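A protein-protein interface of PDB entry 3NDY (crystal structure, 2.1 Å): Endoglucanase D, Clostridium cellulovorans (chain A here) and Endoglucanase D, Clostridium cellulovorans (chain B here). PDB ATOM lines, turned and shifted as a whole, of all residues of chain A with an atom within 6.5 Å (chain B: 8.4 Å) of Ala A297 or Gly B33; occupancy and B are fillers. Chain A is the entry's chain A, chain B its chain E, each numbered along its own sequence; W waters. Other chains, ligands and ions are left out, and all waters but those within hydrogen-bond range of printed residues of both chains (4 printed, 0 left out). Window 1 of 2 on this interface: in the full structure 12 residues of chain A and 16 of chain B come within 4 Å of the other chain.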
ATOM      1  N   TYR A 258      28.149   2.529  31.063  1.00  0.00           N
ATOM      2  CA  TYR A 258      28.900   1.288  31.021  1.00  0.00           C
ATOM      3  C   TYR A 258      30.346   1.494  31.479  1.00  0.00           C
ATOM      4  O   TYR A 258      30.833   0.764  32.336  1.00  0.00           O
ATOM      5  CB  TYR A 258      28.872   0.671  29.613  1.00  0.00           C
ATOM      6  CG  TYR A 258      29.552  -0.685  29.548  1.00  0.00           C
ATOM      7  CD1 TYR A 258      30.884  -0.810  29.139  1.00  0.00           C
ATOM      8  CD2 TYR A 258      28.876  -1.835  29.920  1.00  0.00           C
ATOM      9  CE1 TYR A 258      31.513  -2.056  29.092  1.00  0.00           C
ATOM     10  CE2 TYR A 258      29.494  -3.086  29.869  1.00  0.00           C
ATOM     11  CZ  TYR A 258      30.808  -3.189  29.458  1.00  0.00           C
ATOM     12  OH  TYR A 258      31.410  -4.432  29.422  1.00  0.00           O
ATOM     13  N   ALA A 292      15.785  -0.711  24.458  1.00  0.00           N
ATOM     14  CA  ALA A 292      15.869  -1.952  25.216  1.00  0.00           C
ATOM     15  C   ALA A 292      17.107  -2.783  24.855  1.00  0.00           C
ATOM     16  O   ALA A 292      17.824  -3.232  25.734  1.00  0.00           O
ATOM     17  CB  ALA A 292      14.572  -2.782  25.053  1.00  0.00           C
ATOM     18  N   LYS A 293      17.375  -2.986  23.571  1.00  0.00           N
ATOM     19  CA  LYS A 293      18.529  -3.803  23.214  1.00  0.00           C
ATOM     20  C   LYS A 293      19.860  -3.075  23.432  1.00  0.00           C
ATOM     21  O   LYS A 293      20.854  -3.693  23.801  1.00  0.00           O
ATOM     22  CB  LYS A 293      18.428  -4.316  21.771  1.00  0.00           C
ATOM     23  CG  LYS A 293      18.596  -3.253  20.719  1.00  0.00           C
ATOM     24  CD  LYS A 293      18.698  -3.862  19.324  1.00  0.00           C
ATOM     25  CE  LYS A 293      17.879  -5.125  19.218  1.00  0.00           C
ATOM     26  NZ  LYS A 293      16.444  -4.867  19.512  1.00  0.00           N
ATOM     27  N   SER A 294      19.881  -1.766  23.204  1.00  0.00           N
ATOM     28  CA  SER A 294      21.108  -1.000  23.391  1.00  0.00           C
ATOM     29  C   SER A 294      21.469  -0.947  24.873  1.00  0.00           C
ATOM     30  O   SER A 294      22.634  -1.128  25.241  1.00  0.00           O
ATOM     31  CB  SER A 294      20.981   0.409  22.800  1.00  0.00           C
ATOM     32  OG  SER A 294      22.158   1.168  23.016  1.00  0.00           O
ATOM     33  N   ALA A 295      20.469  -0.710  25.718  1.00  0.00           N
ATOM     34  CA  ALA A 295      20.681  -0.655  27.165  1.00  0.00           C
ATOM     35  C   ALA A 295      21.123  -2.007  27.717  1.00  0.00           C
ATOM     36  O   ALA A 295      22.073  -2.086  28.496  1.00  0.00           O
ATOM     37  CB  ALA A 295      19.412  -0.193  27.866  1.00  0.00           C
ATOM     38  N   LYS A 296      20.425  -3.072  27.319  1.00  0.00           N
ATOM     39  CA  LYS A 296      20.768  -4.408  27.790  1.00  0.00           C
ATOM     40  C   LYS A 296      22.195  -4.798  27.373  1.00  0.00           C
ATOM     41  O   LYS A 296      22.914  -5.455  28.137  1.00  0.00           O
ATOM     42  CB  LYS A 296      19.750  -5.445  27.303  1.00  0.00           C
ATOM     43  CG  LYS A 296      19.986  -6.852  27.847  1.00  0.00           C
ATOM     44  CD  LYS A 296      19.867  -6.919  29.398  1.00  0.00           C
ATOM     45  CE  LYS A 296      18.545  -6.348  29.906  1.00  0.00           C
ATOM     46  NZ  LYS A 296      18.410  -6.514  31.400  1.00  0.00           N
ATOM     47  N   ALA A 297      22.618  -4.377  26.181  1.00  0.00           N
ATOM     48  CA  ALA A 297      23.991  -4.660  25.736  1.00  0.00           C
ATOM     49  C   ALA A 297      25.050  -3.966  26.601  1.00  0.00           C
ATOM     50  O   ALA A 297      26.230  -4.304  26.532  1.00  0.00           O
ATOM     51  CB  ALA A 297      24.191  -4.303  24.263  1.00  0.00           C
ATOM     52  N   ARG A 298      24.638  -2.989  27.404  1.00  0.00           N
ATOM     53  CA  ARG A 298      25.565  -2.389  28.355  1.00  0.00           C
ATOM     54  C   ARG A 298      25.250  -2.852  29.765  1.00  0.00           C
ATOM     55  O   ARG A 298      25.673  -2.220  30.723  1.00  0.00           O
ATOM     56  CB  ARG A 298      25.527  -0.862  28.305  1.00  0.00           C
ATOM     57  CG  ARG A 298      26.302  -0.241  27.153  1.00  0.00           C
ATOM     58  CD  ARG A 298      25.472  -0.195  25.902  1.00  0.00           C
ATOM     59  NE  ARG A 298      26.203   0.334  24.752  1.00  0.00           N
ATOM     60  CZ  ARG A 298      25.829   0.120  23.496  1.00  0.00           C
ATOM     61  NH1 ARG A 298      24.743  -0.601  23.253  1.00  0.00           N
ATOM     62  NH2 ARG A 298      26.541   0.605  22.489  1.00  0.00           N
ATOM     63  N   GLY A 299      24.490  -3.939  29.890  1.00  0.00           N
ATOM     64  CA  GLY A 299      24.212  -4.516  31.197  1.00  0.00           C
ATOM     65  C   GLY A 299      23.146  -3.797  32.006  1.00  0.00           C
ATOM     66  O   GLY A 299      22.948  -4.097  33.177  1.00  0.00           O
ATOM     67  N   LEU A 300      22.441  -2.867  31.372  1.00  0.00           N
ATOM     68  CA  LEU A 300      21.476  -2.023  32.073  1.00  0.00           C
ATOM     69  C   LEU A 300      20.080  -2.637  32.005  1.00  0.00           C
ATOM     70  O   LEU A 300      19.679  -3.208  30.980  1.00  0.00           O
ATOM     71  CB  LEU A 300      21.467  -0.611  31.472  1.00  0.00           C
ATOM     72  CG  LEU A 300      22.851   0.048  31.335  1.00  0.00           C
ATOM     73  CD1 LEU A 300      22.779   1.420  30.644  1.00  0.00           C
ATOM     74  CD2 LEU A 300      23.526   0.172  32.701  1.00  0.00           C
ATOM     75  N   PRO B  30      39.427  -2.884  23.147  1.00  0.00           N
ATOM     76  CA  PRO B  30      38.463  -3.715  23.875  1.00  0.00           C
ATOM     77  C   PRO B  30      37.038  -3.574  23.304  1.00  0.00           C
ATOM     78  O   PRO B  30      36.639  -2.498  22.825  1.00  0.00           O
ATOM     79  CB  PRO B  30      38.528  -3.162  25.306  1.00  0.00           C
ATOM     80  CG  PRO B  30      39.875  -2.473  25.399  1.00  0.00           C
ATOM     81  CD  PRO B  30      40.088  -1.892  24.014  1.00  0.00           C
ATOM     82  N   ILE B  31      36.286  -4.672  23.336  1.00  0.00           N
ATOM     83  CA  ILE B  31      34.895  -4.660  22.910  1.00  0.00           C
ATOM     84  C   ILE B  31      34.026  -4.423  24.148  1.00  0.00           C
ATOM     85  O   ILE B  31      33.838  -5.326  24.970  1.00  0.00           O
ATOM     86  CB  ILE B  31      34.521  -5.980  22.177  1.00  0.00           C
ATOM     87  CG1 ILE B  31      35.334  -6.122  20.887  1.00  0.00           C
ATOM     88  CG2 ILE B  31      33.018  -6.028  21.859  1.00  0.00           C
ATOM     89  CD1 ILE B  31      35.230  -7.521  20.210  1.00  0.00           C
ATOM     90  N   ASN B  32      33.538  -3.191  24.303  1.00  0.00           N
ATOM     91  CA  ASN B  32      32.802  -2.799  25.508  1.00  0.00           C
ATOM     92  C   ASN B  32      31.297  -3.023  25.432  1.00  0.00           C
ATOM     93  O   ASN B  32      30.539  -2.095  25.141  1.00  0.00           O
ATOM     94  CB  ASN B  32      33.087  -1.341  25.864  1.00  0.00           C
ATOM     95  CG  ASN B  32      34.474  -1.151  26.400  1.00  0.00           C
ATOM     96  OD1 ASN B  32      34.917  -1.916  27.249  1.00  0.00           O
ATOM     97  ND2 ASN B  32      35.179  -0.138  25.905  1.00  0.00           N
ATOM     98  N   GLY B  33      30.870  -4.248  25.714  1.00  0.00           N
ATOM     99  CA  GLY B  33      29.462  -4.596  25.667  1.00  0.00           C
ATOM    100  C   GLY B  33      29.184  -5.401  24.415  1.00  0.00           C
ATOM    101  O   GLY B  33      28.481  -4.947  23.516  1.00  0.00           O
ATOM    102  N   TRP B  34      29.741  -6.606  24.357  1.00  0.00           N
ATOM    103  CA  TRP B  34      29.659  -7.392  23.131  1.00  0.00           C
ATOM    104  C   TRP B  34      28.241  -7.871  22.823  1.00  0.00           C
ATOM    105  O   TRP B  34      27.422  -8.098  23.726  1.00  0.00           O
ATOM    106  CB  TRP B  34      30.630  -8.576  23.164  1.00  0.00           C
ATOM    107  CG  TRP B  34      30.329  -9.625  24.211  1.00  0.00           C
ATOM    108  CD1 TRP B  34      30.900  -9.738  25.449  1.00  0.00           C
ATOM    109  CD2 TRP B  34      29.410 -10.726  24.094  1.00  0.00           C
ATOM    110  NE1 TRP B  34      30.392 -10.833  26.108  1.00  0.00           N
ATOM    111  CE2 TRP B  34      29.477 -11.458  25.299  1.00  0.00           C
ATOM    112  CE3 TRP B  34      28.539 -11.161  23.090  1.00  0.00           C
ATOM    113  CZ2 TRP B  34      28.693 -12.594  25.534  1.00  0.00           C
ATOM    114  CZ3 TRP B  34      27.769 -12.302  23.317  1.00  0.00           C
ATOM    115  CH2 TRP B  34      27.850 -13.002  24.534  1.00  0.00           C
ATOM    116  N   THR B  35      27.964  -7.985  21.530  1.00  0.00           N
ATOM    117  CA  THR B  35      26.780  -8.659  21.029  1.00  0.00           C
ATOM    118  C   THR B  35      27.264  -9.547  19.890  1.00  0.00           C
ATOM    119  O   THR B  35      28.267  -9.244  19.239  1.00  0.00           O
ATOM    120  CB  THR B  35      25.754  -7.676  20.485  1.00  0.00           C
ATOM    121  OG1 THR B  35      26.384  -6.842  19.500  1.00  0.00           O
ATOM    122  CG2 THR B  35      25.192  -6.811  21.614  1.00  0.00           C
ATOM    123  N   LEU B  36      26.573 -10.657  19.676  1.00  0.00           N
ATOM    124  CA  LEU B  36      26.987 -11.634  18.687  1.00  0.00           C
ATOM    125  C   LEU B  36      25.763 -12.098  17.920  1.00  0.00           C
ATOM    126  O   LEU B  36      24.756 -12.478  18.508  1.00  0.00           O
ATOM    127  CB  LEU B  36      27.653 -12.832  19.365  1.00  0.00           C
ATOM    128  CG  LEU B  36      28.021 -14.010  18.468  1.00  0.00           C
ATOM    129  CD1 LEU B  36      29.118 -13.630  17.489  1.00  0.00           C
ATOM    130  CD2 LEU B  36      28.455 -15.218  19.315  1.00  0.00           C
ATOM    131  N   SER B  53      21.949 -13.508  26.961  1.00  0.00           N
ATOM    132  CA  SER B  53      20.535 -13.572  26.591  1.00  0.00           C
ATOM    133  C   SER B  53      20.406 -13.452  25.074  1.00  0.00           C
ATOM    134  O   SER B  53      21.373 -13.136  24.387  1.00  0.00           O
ATOM    135  CB  SER B  53      19.726 -12.483  27.315  1.00  0.00           C
ATOM    136  OG  SER B  53      20.120 -11.176  26.921  1.00  0.00           O
ATOM    137  N   VAL B  63      22.567 -12.506  20.159  1.00  0.00           N
ATOM    138  CA  VAL B  63      22.970 -12.784  21.533  1.00  0.00           C
ATOM    139  C   VAL B  63      23.603 -11.545  22.157  1.00  0.00           C
ATOM    140  O   VAL B  63      24.375 -10.832  21.503  1.00  0.00           O
ATOM    141  CB  VAL B  63      23.978 -13.948  21.606  1.00  0.00           C
ATOM    142  CG1 VAL B  63      24.397 -14.210  23.064  1.00  0.00           C
ATOM    143  CG2 VAL B  63      23.390 -15.217  20.964  1.00  0.00           C
ATOM    144  N   THR B  64      23.270 -11.296  23.421  1.00  0.00           N
ATOM    145  CA  THR B  64      23.794 -10.150  24.158  1.00  0.00           C
ATOM    146  C   THR B  64      24.468 -10.610  25.449  1.00  0.00           C
ATOM    147  O   THR B  64      23.964 -11.494  26.151  1.00  0.00           O
ATOM    148  CB  THR B  64      22.672  -9.137  24.484  1.00  0.00           C
ATOM    149  OG1 THR B  64      22.117  -8.626  23.264  1.00  0.00           O
ATOM    150  CG2 THR B  64      23.204  -7.981  25.310  1.00  0.00           C
ATOM    151  N   ASN B  65      25.612 -10.009  25.753  1.00  0.00           N
ATOM    152  CA  ASN B  65      26.331 -10.292  26.990  1.00  0.00           C
ATOM    153  C   ASN B  65      25.460 -10.139  28.252  1.00  0.00           C
ATOM    154  O   ASN B  65      24.373  -9.548  28.212  1.00  0.00           O
ATOM    155  CB  ASN B  65      27.548  -9.373  27.089  1.00  0.00           C
ATOM    156  CG  ASN B  65      27.158  -7.947  27.424  1.00  0.00           C
ATOM    157  OD1 ASN B  65      26.930  -7.620  28.590  1.00  0.00           O
ATOM    158  ND2 ASN B  65      27.069  -7.093  26.403  1.00  0.00           N
ATOM    159  N   ALA B  66      25.956 -10.663  29.374  1.00  0.00           N
ATOM    160  CA  ALA B  66      25.228 -10.623  30.640  1.00  0.00           C
ATOM    161  C   ALA B  66      25.781  -9.564  31.601  1.00  0.00           C
ATOM    162  O   ALA B  66      25.575  -9.644  32.813  1.00  0.00           O
ATOM    163  CB  ALA B  66      25.248 -11.994  31.296  1.00  0.00           C
ATOM    164  N   GLY B  67      26.496  -8.581  31.061  1.00  0.00           N
ATOM    165  CA  GLY B  67      26.946  -7.454  31.862  1.00  0.00           C
ATOM    166  C   GLY B  67      28.268  -7.701  32.559  1.00  0.00           C
ATOM    167  O   GLY B  67      29.247  -6.998  32.286  1.00  0.00           O
ATOM    168  N   ASN B  69      30.166 -10.019  32.048  1.00  0.00           N
ATOM    169  CA  ASN B  69      31.101 -10.494  31.029  1.00  0.00           C
ATOM    170  C   ASN B  69      31.037  -9.662  29.748  1.00  0.00           C
ATOM    171  O   ASN B  69      31.366 -10.156  28.675  1.00  0.00           O
ATOM    172  CB  ASN B  69      30.858 -11.982  30.718  1.00  0.00           C
ATOM    173  CG  ASN B  69      29.468 -12.243  30.175  1.00  0.00           C
ATOM    174  OD1 ASN B  69      28.656 -11.328  30.060  1.00  0.00           O
ATOM    175  ND2 ASN B  69      29.193 -13.493  29.824  1.00  0.00           N
ATOM    176  N   GLY B  70      30.636  -8.396  29.862  1.00  0.00           N
ATOM    177  CA  GLY B  70      30.374  -7.587  28.681  1.00  0.00           C
ATOM    178  C   GLY B  70      31.589  -7.074  27.916  1.00  0.00           C
ATOM    179  O   GLY B  70      31.497  -6.783  26.717  1.00  0.00           O
ATOM    180  N   THR B  71      32.732  -6.965  28.590  1.00  0.00           N
ATOM    181  CA  THR B  71      33.947  -6.469  27.932  1.00  0.00           C
ATOM    182  C   THR B  71      34.885  -7.575  27.473  1.00  0.00           C
ATOM    183  O   THR B  71      35.389  -8.345  28.288  1.00  0.00           O
ATOM    184  CB  THR B  71      34.759  -5.523  28.838  1.00  0.00           C
ATOM    185  OG1 THR B  71      33.987  -4.358  29.132  1.00  0.00           O
ATOM    186  CG2 THR B  71      36.057  -5.101  28.140  1.00  0.00           C
ATOM    187  N   ILE B  72      35.130  -7.649  26.168  1.00  0.00           N
ATOM    188  CA  ILE B  72      36.126  -8.583  25.668  1.00  0.00           C
ATOM    189  C   ILE B  72      37.438  -7.824  25.493  1.00  0.00           C
ATOM    190  O   ILE B  72      37.563  -6.964  24.610  1.00  0.00           O
ATOM    191  CB  ILE B  72      35.704  -9.248  24.335  1.00  0.00           C
ATOM    192  CG1 ILE B  72      34.209  -9.599  24.349  1.00  0.00           C
ATOM    193  CG2 ILE B  72      36.559 -10.484  24.059  1.00  0.00           C
ATOM    194  CD1 ILE B  72      33.728 -10.368  23.131  1.00  0.00           C
ATOM    195  N   GLN B  79      35.460 -14.019  26.108  1.00  0.00           N
ATOM    196  CA  GLN B  79      34.281 -14.172  26.940  1.00  0.00           C
ATOM    197  C   GLN B  79      33.517 -15.348  26.327  1.00  0.00           C
ATOM    198  O   GLN B  79      33.630 -15.600  25.139  1.00  0.00           O
ATOM    199  CB  GLN B  79      33.419 -12.904  26.941  1.00  0.00           C
ATOM    200  CG  GLN B  79      34.054 -11.671  27.612  1.00  0.00           C
ATOM    201  CD  GLN B  79      34.235 -11.816  29.119  1.00  0.00           C
ATOM    202  OE1 GLN B  79      33.874 -12.834  29.717  1.00  0.00           O
ATOM    203  NE2 GLN B  79      34.809 -10.795  29.738  1.00  0.00           N
ATOM    204  N   VAL B  99      30.266  -9.723  15.451  1.00  0.00           N
ATOM    205  CA  VAL B  99      30.366  -9.214  16.812  1.00  0.00           C
ATOM    206  C   VAL B  99      30.390  -7.701  16.698  1.00  0.00           C
ATOM    207  O   VAL B  99      31.291  -7.142  16.081  1.00  0.00           O
ATOM    208  CB  VAL B  99      31.643  -9.717  17.528  1.00  0.00           C
ATOM    209  CG1 VAL B  99      31.812  -9.029  18.881  1.00  0.00           C
ATOM    210  CG2 VAL B  99      31.589 -11.224  17.712  1.00  0.00           C
ATOM    211  N   ASN B 100      29.387  -7.050  17.277  1.00  0.00           N
ATOM    212  CA  ASN B 100      29.211  -5.611  17.113  1.00  0.00           C
ATOM    213  C   ASN B 100      29.459  -5.117  15.687  1.00  0.00           C
ATOM    214  O   ASN B 100      30.170  -4.131  15.471  1.00  0.00           O
ATOM    215  CB  ASN B 100      30.086  -4.863  18.113  1.00  0.00           C
ATOM    216  CG  ASN B 100      29.785  -5.263  19.540  1.00  0.00           C
ATOM    217  OD1 ASN B 100      29.910  -6.432  19.908  1.00  0.00           O
ATOM    218  ND2 ASN B 100      29.371  -4.304  20.346  1.00  0.00           N
HETATM  219  O   HOH W   1      31.608  -5.833  32.512  1.00  0.00           O
HETATM  220  O   HOH W   2      27.609  -2.477  22.923  1.00  0.00           O
HETATM  221  O   HOH W   3      23.351  -7.542  29.782  1.00  0.00           O
HETATM  222  O   HOH W   4      20.812  -6.357  23.165  1.00  0.00           O
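The side-chain hydroxyl of Tyr A258 lies within hydrogen-bond range of the side-chain hydroxyl of Thr B71.
O of Ala A297 sits at hydrogen-bond distance from ND2 of Asn B65.
OD1 of Asn B32 sits at hydrogen-bond distance from OG1 of Thr B71 (3.2 Å).
The backbone NH (N) of Thr B35 is in hydrogen-bond range of the side-chain amide oxygen (OD1) of Asn B100 (3.0 Å).
O of Ser B53 lies within hydrogen-bond range of N of Thr B64, at 2.8 Å.
The backbone NH (N) of Gly B67 lies within hydrogen-bond range of the side-chain amide oxygen (OD1) of Asn B65 (2.7 Å).
O of Thr B71 sits at hydrogen-bond distance from NE2 of Gln B79, 2.9 Å away.
The backbone carbonyl oxygen (O) of Gly B33 is in hydrogen-bond range of the side-chain amide nitrogen (ND2) of Asn B100, at 3.4 Å.
Among the printed residues, pairs that only touch across the chains: Tyr A258 with Asn B32, Tyr A258 with Gly B33, Tyr A258 with Gly B70, Lys A296 with Thr B64, Ala A297 with Gly B33, Ala A297 with Thr B35 and Ala A297 with Thr B64.
Ala A295 touches none of the printed residues of chain B.
Printed residues of chain B within 4 Å of Lys A296: Thr B64 (3.8 Å).
Ala A297 touches just these residues of chain B: Gly B33 (3.4 Å), Thr B35 (3.8 Å), Thr B64 (3.4 Å) and Asn B65 (2.9 Å).
Printed residues of chain A within 4 Å of Asn B32: Tyr A258 (3.7 Å).
Of chain A, only Tyr A258 (3.8 Å) and Ala A297 (3.4 Å) come within 4 Å of Gly B33.
Of the printed residues of chain A, Thr B35 touches Ala A297.
Leu B36 touches none of the printed residues of chain A.
Of the printed residues of chain A, Thr B64 touches Lys A296 (3.8 Å) and Ala A297 (3.4 Å).
Printed residues of chain A within 4 Å of Asn B65: Ala A297 (2.9 Å).
The nearest residue of chain B that does not touch Ala A297 is Trp B34 (4.7 Å).
The nearest printed residue of chain A that does not touch Asn B32 is Arg A298 (5.0 Å).
Of the 10 printed residues of chain A, 3 touch a printed residue of chain B.
Hydrophobic or aromatic side chains of chain A that line the printed part of chain B: Tyr A258 and Ala A297.
Among the printed residues, 9 pairs touch across the chains.
Among the printed residues, no Asp or Glu carboxylate lies within 4 Å of a Lys or Arg side-chain nitrogen of the other chain.
Water W4 bridges OG1 of Thr B64 and O of Lys A293.
Water W1 lies within hydrogen-bond range of the backbone carbonyl oxygen of Gly B67 (2.6 Å) and the side-chain hydroxyl of Tyr A258 (3.4 Å).
Water W2 bridges the backbone carbonyl oxygen (O) of Gly B33 and the guanidinium group (NH2) of Arg A298.
Water W3 lies within hydrogen-bond range of O of Lys A296 and O of Asn B65.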
